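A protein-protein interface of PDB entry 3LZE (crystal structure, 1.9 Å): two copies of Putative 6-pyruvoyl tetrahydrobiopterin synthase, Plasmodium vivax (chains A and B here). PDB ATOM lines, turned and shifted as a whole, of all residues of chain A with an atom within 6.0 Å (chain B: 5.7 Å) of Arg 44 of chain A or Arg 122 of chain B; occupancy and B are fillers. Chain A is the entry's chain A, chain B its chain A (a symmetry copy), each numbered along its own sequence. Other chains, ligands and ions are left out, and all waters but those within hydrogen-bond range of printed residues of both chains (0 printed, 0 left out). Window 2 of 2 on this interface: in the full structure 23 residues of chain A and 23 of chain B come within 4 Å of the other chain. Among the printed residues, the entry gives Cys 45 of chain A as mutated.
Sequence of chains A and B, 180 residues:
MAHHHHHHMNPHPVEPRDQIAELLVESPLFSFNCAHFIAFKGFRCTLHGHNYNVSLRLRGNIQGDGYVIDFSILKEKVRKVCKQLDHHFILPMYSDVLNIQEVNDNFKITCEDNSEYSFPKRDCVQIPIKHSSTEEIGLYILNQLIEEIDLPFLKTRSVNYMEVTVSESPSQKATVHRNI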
ATOM      1  N   PHE A  37      -4.505  23.080  -9.036  1.00  0.00           N
ATOM      2  CA  PHE A  37      -3.307  22.577  -9.616  1.00  0.00           C
ATOM      3  C   PHE A  37      -2.637  23.779 -10.235  1.00  0.00           C
ATOM      4  O   PHE A  37      -3.301  24.693 -10.650  1.00  0.00           O
ATOM      5  CB  PHE A  37      -3.543  21.411 -10.622  1.00  0.00           C
ATOM      6  CG  PHE A  37      -4.297  21.792 -11.915  1.00  0.00           C
ATOM      7  CD1 PHE A  37      -3.617  22.337 -13.000  1.00  0.00           C
ATOM      8  CD2 PHE A  37      -5.622  21.396 -12.099  1.00  0.00           C
ATOM      9  CE1 PHE A  37      -4.290  22.605 -14.227  1.00  0.00           C
ATOM     10  CE2 PHE A  37      -6.299  21.648 -13.290  1.00  0.00           C
ATOM     11  CZ  PHE A  37      -5.619  22.284 -14.363  1.00  0.00           C
ATOM     12  N   ILE A  38      -1.318  23.734 -10.281  1.00  0.00           N
ATOM     13  CA  ILE A  38      -0.484  24.807 -10.823  1.00  0.00           C
ATOM     14  C   ILE A  38      -0.219  24.533 -12.278  1.00  0.00           C
ATOM     15  O   ILE A  38       0.144  23.421 -12.634  1.00  0.00           O
ATOM     16  CB  ILE A  38       0.885  24.869 -10.086  1.00  0.00           C
ATOM     17  CG1 ILE A  38       0.684  25.239  -8.613  1.00  0.00           C
ATOM     18  CG2 ILE A  38       1.845  25.873 -10.757  1.00  0.00           C
ATOM     19  CD1 ILE A  38       0.007  26.585  -8.402  1.00  0.00           C
ATOM     20  N   ALA A  39      -0.396  25.541 -13.120  1.00  0.00           N
ATOM     21  CA  ALA A  39      -0.040  25.457 -14.512  1.00  0.00           C
ATOM     22  C   ALA A  39       0.451  26.857 -14.856  1.00  0.00           C
ATOM     23  O   ALA A  39      -0.175  27.846 -14.463  1.00  0.00           O
ATOM     24  CB  ALA A  39      -1.243  25.083 -15.368  1.00  0.00           C
ATOM     25  N   PHE A  40       1.613  26.910 -15.498  1.00  0.00           N
ATOM     26  CA  PHE A  40       2.132  28.100 -16.138  1.00  0.00           C
ATOM     27  C   PHE A  40       2.974  27.614 -17.324  1.00  0.00           C
ATOM     28  O   PHE A  40       3.161  26.407 -17.501  1.00  0.00           O
ATOM     29  CB  PHE A  40       2.946  28.964 -15.146  1.00  0.00           C
ATOM     30  CG  PHE A  40       4.041  28.224 -14.420  1.00  0.00           C
ATOM     31  CD1 PHE A  40       5.313  28.057 -15.013  1.00  0.00           C
ATOM     32  CD2 PHE A  40       3.839  27.764 -13.112  1.00  0.00           C
ATOM     33  CE1 PHE A  40       6.340  27.391 -14.333  1.00  0.00           C
ATOM     34  CE2 PHE A  40       4.856  27.087 -12.426  1.00  0.00           C
ATOM     35  CZ  PHE A  40       6.112  26.899 -13.034  1.00  0.00           C
ATOM     36  N   GLY A  42       5.035  25.998 -19.956  1.00  0.00           N
ATOM     37  CA  GLY A  42       5.975  24.885 -19.899  1.00  0.00           C
ATOM     38  C   GLY A  42       5.906  24.046 -18.638  1.00  0.00           C
ATOM     39  O   GLY A  42       6.799  23.227 -18.394  1.00  0.00           O
ATOM     40  N   PHE A  43       4.850  24.228 -17.834  1.00  0.00           N
ATOM     41  CA  PHE A  43       4.702  23.469 -16.595  1.00  0.00           C
ATOM     42  C   PHE A  43       3.234  23.254 -16.175  1.00  0.00           C
ATOM     43  O   PHE A  43       2.411  24.178 -16.243  1.00  0.00           O
ATOM     44  CB  PHE A  43       5.484  24.140 -15.453  1.00  0.00           C
ATOM     45  CG  PHE A  43       5.472  23.332 -14.185  1.00  0.00           C
ATOM     46  CD1 PHE A  43       6.375  22.280 -14.003  1.00  0.00           C
ATOM     47  CD2 PHE A  43       4.541  23.597 -13.192  1.00  0.00           C
ATOM     48  CE1 PHE A  43       6.344  21.499 -12.836  1.00  0.00           C
ATOM     49  CE2 PHE A  43       4.484  22.808 -12.019  1.00  0.00           C
ATOM     50  CZ  PHE A  43       5.396  21.770 -11.837  1.00  0.00           C
ATOM     51  N   ARG A  44       2.940  22.032 -15.729  1.00  0.00           N
ATOM     52  CA  ARG A  44       1.616  21.648 -15.202  1.00  0.00           C
ATOM     53  C   ARG A  44       1.845  20.656 -14.058  1.00  0.00           C
ATOM     54  O   ARG A  44       2.505  19.628 -14.261  1.00  0.00           O
ATOM     55  CB  ARG A  44       0.775  20.998 -16.313  1.00  0.00           C
ATOM     56  CG  ARG A  44      -0.708  20.778 -16.006  1.00  0.00           C
ATOM     57  CD  ARG A  44      -1.002  19.423 -15.401  1.00  0.00           C
ATOM     58  NE  ARG A  44      -0.793  18.285 -16.313  1.00  0.00           N
ATOM     59  CZ  ARG A  44      -1.138  17.024 -16.022  1.00  0.00           C
ATOM     60  NH1 ARG A  44      -1.719  16.725 -14.860  1.00  0.00           N
ATOM     61  NH2 ARG A  44      -0.905  16.051 -16.891  1.00  0.00           N
ATOM     62  N   CYS A  45       1.332  20.934 -12.861  1.00  0.00           N
ATOM     63  CA  CYS A  45       1.373  19.907 -11.811  1.00  0.00           C
ATOM     64  C   CYS A  45       0.062  19.138 -11.840  1.00  0.00           C
ATOM     65  O   CYS A  45      -0.905  19.517 -12.520  1.00  0.00           O
ATOM     66  CB  CYS A  45       1.587  20.486 -10.412  1.00  0.00           C
ATOM     67  SG  CYS A  45       0.050  20.876  -9.499  1.00  0.00           S
ATOM     68  N   THR A  46       0.061  18.039 -11.105  1.00  0.00           N
ATOM     69  CA  THR A  46      -1.122  17.224 -10.975  1.00  0.00           C
ATOM     70  C   THR A  46      -2.118  17.882  -9.993  1.00  0.00           C
ATOM     71  O   THR A  46      -1.764  18.690  -9.139  1.00  0.00           O
ATOM     72  CB  THR A  46      -0.745  15.800 -10.489  1.00  0.00           C
ATOM     73  OG1 THR A  46       0.152  15.903  -9.378  1.00  0.00           O
ATOM     74  CG2 THR A  46      -0.006  15.011 -11.586  1.00  0.00           C
ATOM     75  N   LEU A  47      -3.373  17.512 -10.149  1.00  0.00           N
ATOM     76  CA  LEU A  47      -4.405  17.847  -9.208  1.00  0.00           C
ATOM     77  C   LEU A  47      -4.109  17.324  -7.811  1.00  0.00           C
ATOM     78  O   LEU A  47      -3.756  16.151  -7.608  1.00  0.00           O
ATOM     79  CB  LEU A  47      -5.725  17.237  -9.660  1.00  0.00           C
ATOM     80  CG  LEU A  47      -6.958  17.538  -8.815  1.00  0.00           C
ATOM     81  CD1 LEU A  47      -7.306  18.993  -8.932  1.00  0.00           C
ATOM     82  CD2 LEU A  47      -8.121  16.628  -9.317  1.00  0.00           C
ATOM     83  N   CYS A 111      -5.160  21.606 -20.540  1.00  0.00           N
ATOM     84  CA  CYS A 111      -3.841  22.182 -20.312  1.00  0.00           C
ATOM     85  C   CYS A 111      -3.020  22.148 -21.616  1.00  0.00           C
ATOM     86  O   CYS A 111      -3.408  21.480 -22.577  1.00  0.00           O
ATOM     87  CB  CYS A 111      -3.133  21.377 -19.218  1.00  0.00           C
ATOM     88  SG  CYS A 111      -4.077  21.388 -17.709  1.00  0.00           S
ATOM     89  N   ASP A 113      -0.312  20.634 -22.279  1.00  0.00           N
ATOM     90  CA  ASP A 113       0.129  19.252 -22.579  1.00  0.00           C
ATOM     91  C   ASP A 113      -1.033  18.319 -22.979  1.00  0.00           C
ATOM     92  O   ASP A 113      -0.867  17.093 -23.063  1.00  0.00           O
ATOM     93  CB  ASP A 113       0.930  18.678 -21.400  1.00  0.00           C
ATOM     94  CG  ASP A 113       0.062  18.383 -20.164  1.00  0.00           C
ATOM     95  OD1 ASP A 113      -1.171  18.548 -20.212  1.00  0.00           O
ATOM     96  OD2 ASP A 113       0.629  18.010 -19.126  1.00  0.00           O
ATOM     97  N   SER A 115      -3.608  17.567 -21.316  1.00  0.00           N
ATOM     98  CA  SER A 115      -4.298  16.965 -20.165  1.00  0.00           C
ATOM     99  C   SER A 115      -5.689  17.603 -20.031  1.00  0.00           C
ATOM    100  O   SER A 115      -5.868  18.783 -20.222  1.00  0.00           O
ATOM    101  CB  SER A 115      -3.535  17.189 -18.864  1.00  0.00           C
ATOM    102  OG  SER A 115      -2.309  16.487 -18.891  1.00  0.00           O
ATOM    103  N   TYR A 117      -9.435  17.860 -17.670  1.00  0.00           N
ATOM    104  CA  TYR A 117     -10.115  17.726 -16.380  1.00  0.00           C
ATOM    105  C   TYR A 117     -11.537  18.180 -16.611  1.00  0.00           C
ATOM    106  O   TYR A 117     -11.803  19.074 -17.402  1.00  0.00           O
ATOM    107  CB  TYR A 117      -9.511  18.670 -15.301  1.00  0.00           C
ATOM    108  CG  TYR A 117      -8.082  18.406 -15.020  1.00  0.00           C
ATOM    109  CD1 TYR A 117      -7.692  17.625 -13.944  1.00  0.00           C
ATOM    110  CD2 TYR A 117      -7.104  18.923 -15.846  1.00  0.00           C
ATOM    111  CE1 TYR A 117      -6.370  17.343 -13.715  1.00  0.00           C
ATOM    112  CE2 TYR A 117      -5.808  18.682 -15.617  1.00  0.00           C
ATOM    113  CZ  TYR A 117      -5.422  17.908 -14.549  1.00  0.00           C
ATOM    114  OH  TYR A 117      -4.083  17.671 -14.411  1.00  0.00           O
ATOM    115  N   HIS B  88      -1.927  13.995  -5.627  1.00  0.00           N
ATOM    116  CA  HIS B  88      -2.854  13.220  -6.436  1.00  0.00           C
ATOM    117  C   HIS B  88      -4.266  13.380  -5.898  1.00  0.00           C
ATOM    118  O   HIS B  88      -4.467  13.786  -4.747  1.00  0.00           O
ATOM    119  CB  HIS B  88      -2.535  11.710  -6.401  1.00  0.00           C
ATOM    120  CG  HIS B  88      -1.274  11.348  -7.105  1.00  0.00           C
ATOM    121  ND1 HIS B  88      -0.056  11.329  -6.471  1.00  0.00           N
ATOM    122  CD2 HIS B  88      -1.042  10.960  -8.381  1.00  0.00           C
ATOM    123  CE1 HIS B  88       0.879  10.966  -7.330  1.00  0.00           C
ATOM    124  NE2 HIS B  88       0.309  10.749  -8.498  1.00  0.00           N
ATOM    125  N   ASP B 105      -7.275   8.440 -21.444  1.00  0.00           N
ATOM    126  CA  ASP B 105      -6.258   8.380 -20.382  1.00  0.00           C
ATOM    127  C   ASP B 105      -6.758   9.026 -19.102  1.00  0.00           C
ATOM    128  O   ASP B 105      -5.974   9.478 -18.266  1.00  0.00           O
ATOM    129  CB  ASP B 105      -4.987   9.089 -20.877  1.00  0.00           C
ATOM    130  CG  ASP B 105      -4.415   8.427 -22.108  1.00  0.00           C
ATOM    131  OD1 ASP B 105      -4.359   7.197 -22.157  1.00  0.00           O
ATOM    132  OD2 ASP B 105      -4.036   9.167 -23.002  1.00  0.00           O
ATOM    133  N   PRO B 120      -7.166  13.079 -15.411  1.00  0.00           N
ATOM    134  CA  PRO B 120      -6.154  12.208 -15.941  1.00  0.00           C
ATOM    135  C   PRO B 120      -5.848  11.057 -14.950  1.00  0.00           C
ATOM    136  O   PRO B 120      -5.707  11.292 -13.753  1.00  0.00           O
ATOM    137  CB  PRO B 120      -4.925  13.158 -16.123  1.00  0.00           C
ATOM    138  CG  PRO B 120      -5.512  14.521 -16.151  1.00  0.00           C
ATOM    139  CD  PRO B 120      -6.658  14.462 -15.212  1.00  0.00           C
ATOM    140  N   LYS B 121      -5.809   9.823 -15.435  1.00  0.00           N
ATOM    141  CA  LYS B 121      -5.458   8.697 -14.591  1.00  0.00           C
ATOM    142  C   LYS B 121      -4.166   8.948 -13.801  1.00  0.00           C
ATOM    143  O   LYS B 121      -4.108   8.589 -12.638  1.00  0.00           O
ATOM    144  CB  LYS B 121      -5.299   7.384 -15.395  1.00  0.00           C
ATOM    145  CG  LYS B 121      -6.550   6.893 -16.141  1.00  0.00           C
ATOM    146  CD  LYS B 121      -6.196   5.651 -16.976  1.00  0.00           C
ATOM    147  CE  LYS B 121      -7.282   5.225 -17.921  1.00  0.00           C
ATOM    148  NZ  LYS B 121      -6.848   3.996 -18.757  1.00  0.00           N
ATOM    149  N   ARG B 122      -3.168   9.596 -14.423  1.00  0.00           N
ATOM    150  CA  ARG B 122      -1.869   9.838 -13.767  1.00  0.00           C
ATOM    151  C   ARG B 122      -1.961  10.835 -12.603  1.00  0.00           C
ATOM    152  O   ARG B 122      -1.071  10.888 -11.756  1.00  0.00           O
ATOM    153  CB  ARG B 122      -0.848  10.335 -14.784  1.00  0.00           C
ATOM    154  CG  ARG B 122      -1.203  11.705 -15.374  1.00  0.00           C
ATOM    155  CD  ARG B 122      -0.195  12.194 -16.430  1.00  0.00           C
ATOM    156  NE  ARG B 122       1.106  12.584 -15.873  1.00  0.00           N
ATOM    157  CZ  ARG B 122       1.321  13.653 -15.097  1.00  0.00           C
ATOM    158  NH1 ARG B 122       2.547  13.926 -14.661  1.00  0.00           N
ATOM    159  NH2 ARG B 122       0.319  14.439 -14.726  1.00  0.00           N
ATOM    160  N   ASP B 123      -3.040  11.624 -12.560  1.00  0.00           N
ATOM    161  CA  ASP B 123      -3.287  12.566 -11.446  1.00  0.00           C
ATOM    162  C   ASP B 123      -3.985  11.850 -10.275  1.00  0.00           C
ATOM    163  O   ASP B 123      -4.167  12.450  -9.221  1.00  0.00           O
ATOM    164  CB  ASP B 123      -4.210  13.744 -11.830  1.00  0.00           C
ATOM    165  CG  ASP B 123      -3.545  14.808 -12.659  1.00  0.00           C
ATOM    166  OD1 ASP B 123      -2.724  14.491 -13.532  1.00  0.00           O
ATOM    167  OD2 ASP B 123      -3.923  15.985 -12.487  1.00  0.00           O
ATOM    168  N   CYS B 124      -4.316  10.583 -10.435  1.00  0.00           N
ATOM    169  CA  CYS B 124      -5.123   9.852  -9.454  1.00  0.00           C
ATOM    170  C   CYS B 124      -4.281   8.734  -8.863  1.00  0.00           C
ATOM    171  O   CYS B 124      -3.388   8.179  -9.537  1.00  0.00           O
ATOM    172  CB  CYS B 124      -6.352   9.210 -10.088  1.00  0.00           C
ATOM    173  SG  CYS B 124      -7.512  10.423 -10.785  1.00  0.00           S
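The guanidinium group (NH1) of Arg 44 of chain A lies within salt-bridge range of the side-chain carboxylate (OD1) of Asp 123 of chain B (2.8 Å).
O of Leu 47 of chain A sits close to N of His 88 of chain B, at 3.5 Å.
The side-chain carboxylate (OD2) of Asp 123 of chain B sits at hydrogen-bond distance from the backbone NH (N) of Leu 47 of chain A (2.8 Å).
OH of Tyr 117 of chain A lies within hydrogen-bond range of OD2 of Asp 123 of chain B.
The guanidinium group of Arg 44 of chain A sits close to the guanidinium group of Arg 122 of chain B, 3.0 Å away.
NE of Arg 44 of chain A is in salt-bridge range of OD2 of Asp 113 of chain A.
The side-chain hydroxyl of Ser 115 of chain A sits at hydrogen-bond distance from the guanidinium group of Arg 44 of chain A (2.5 Å).
OH of Tyr 117 of chain A is in hydrogen-bond range of NH1 of Arg 44 of chain A (2.6 Å).
The side-chain sulfur (SG) of Cys 124 of chain B is in hydrogen-bond range of the backbone carbonyl oxygen (O) of Pro 120 of chain B (3.6 Å).
OD1 of Asp 123 of chain B lies within salt-bridge range of NH2 of Arg 122 of chain B.
CG2 of Thr 46 of chain A touches NH2 of Arg 122 of chain B, at 3.2 Å.
Thr 46 of chain A touches Asp 123 of chain B.
Pro 120 of chain B touches Tyr 117 of chain A (CD to CE1, 3.3 Å).
Printed residues of chain B within 4 Å of Arg 44 of chain A: Arg 122 (3.0 Å) and Asp 123 (2.8 Å).
Printed residues of chain A within 4 Å of Arg 122 of chain B: Arg 44 (3.0 Å) and Thr 46 (3.2 Å).
Of the printed residues of chain B, Tyr 117 of chain A touches Pro 120 and Asp 123.
Of the printed residues of chain A, His 88 of chain B touches Leu 47.
Cys 124 of chain B touches none of the printed residues of chain A.
Of the 14 printed residues of chain A, 4 touch a printed residue of chain B.
Printed residues of chain A that touch a printed residue of chain B: Arg 44, Thr 46, Leu 47 and Tyr 117.
Of the 7 printed residues of chain B, 4 touch a printed residue of chain A.
Printed residues of chain B that touch a printed residue of chain A: His 88, Pro 120, Arg 122 and Asp 123.
Hydrophobic or aromatic side chains of chain B that line the printed part of chain A: Pro 120.
Among the printed residues, 8 pairs touch across the chains.
No position is printed for both chains.
Of the 8 pairs that touch across the chains among the printed residues, none has its exchanged pair printed and touching as well.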
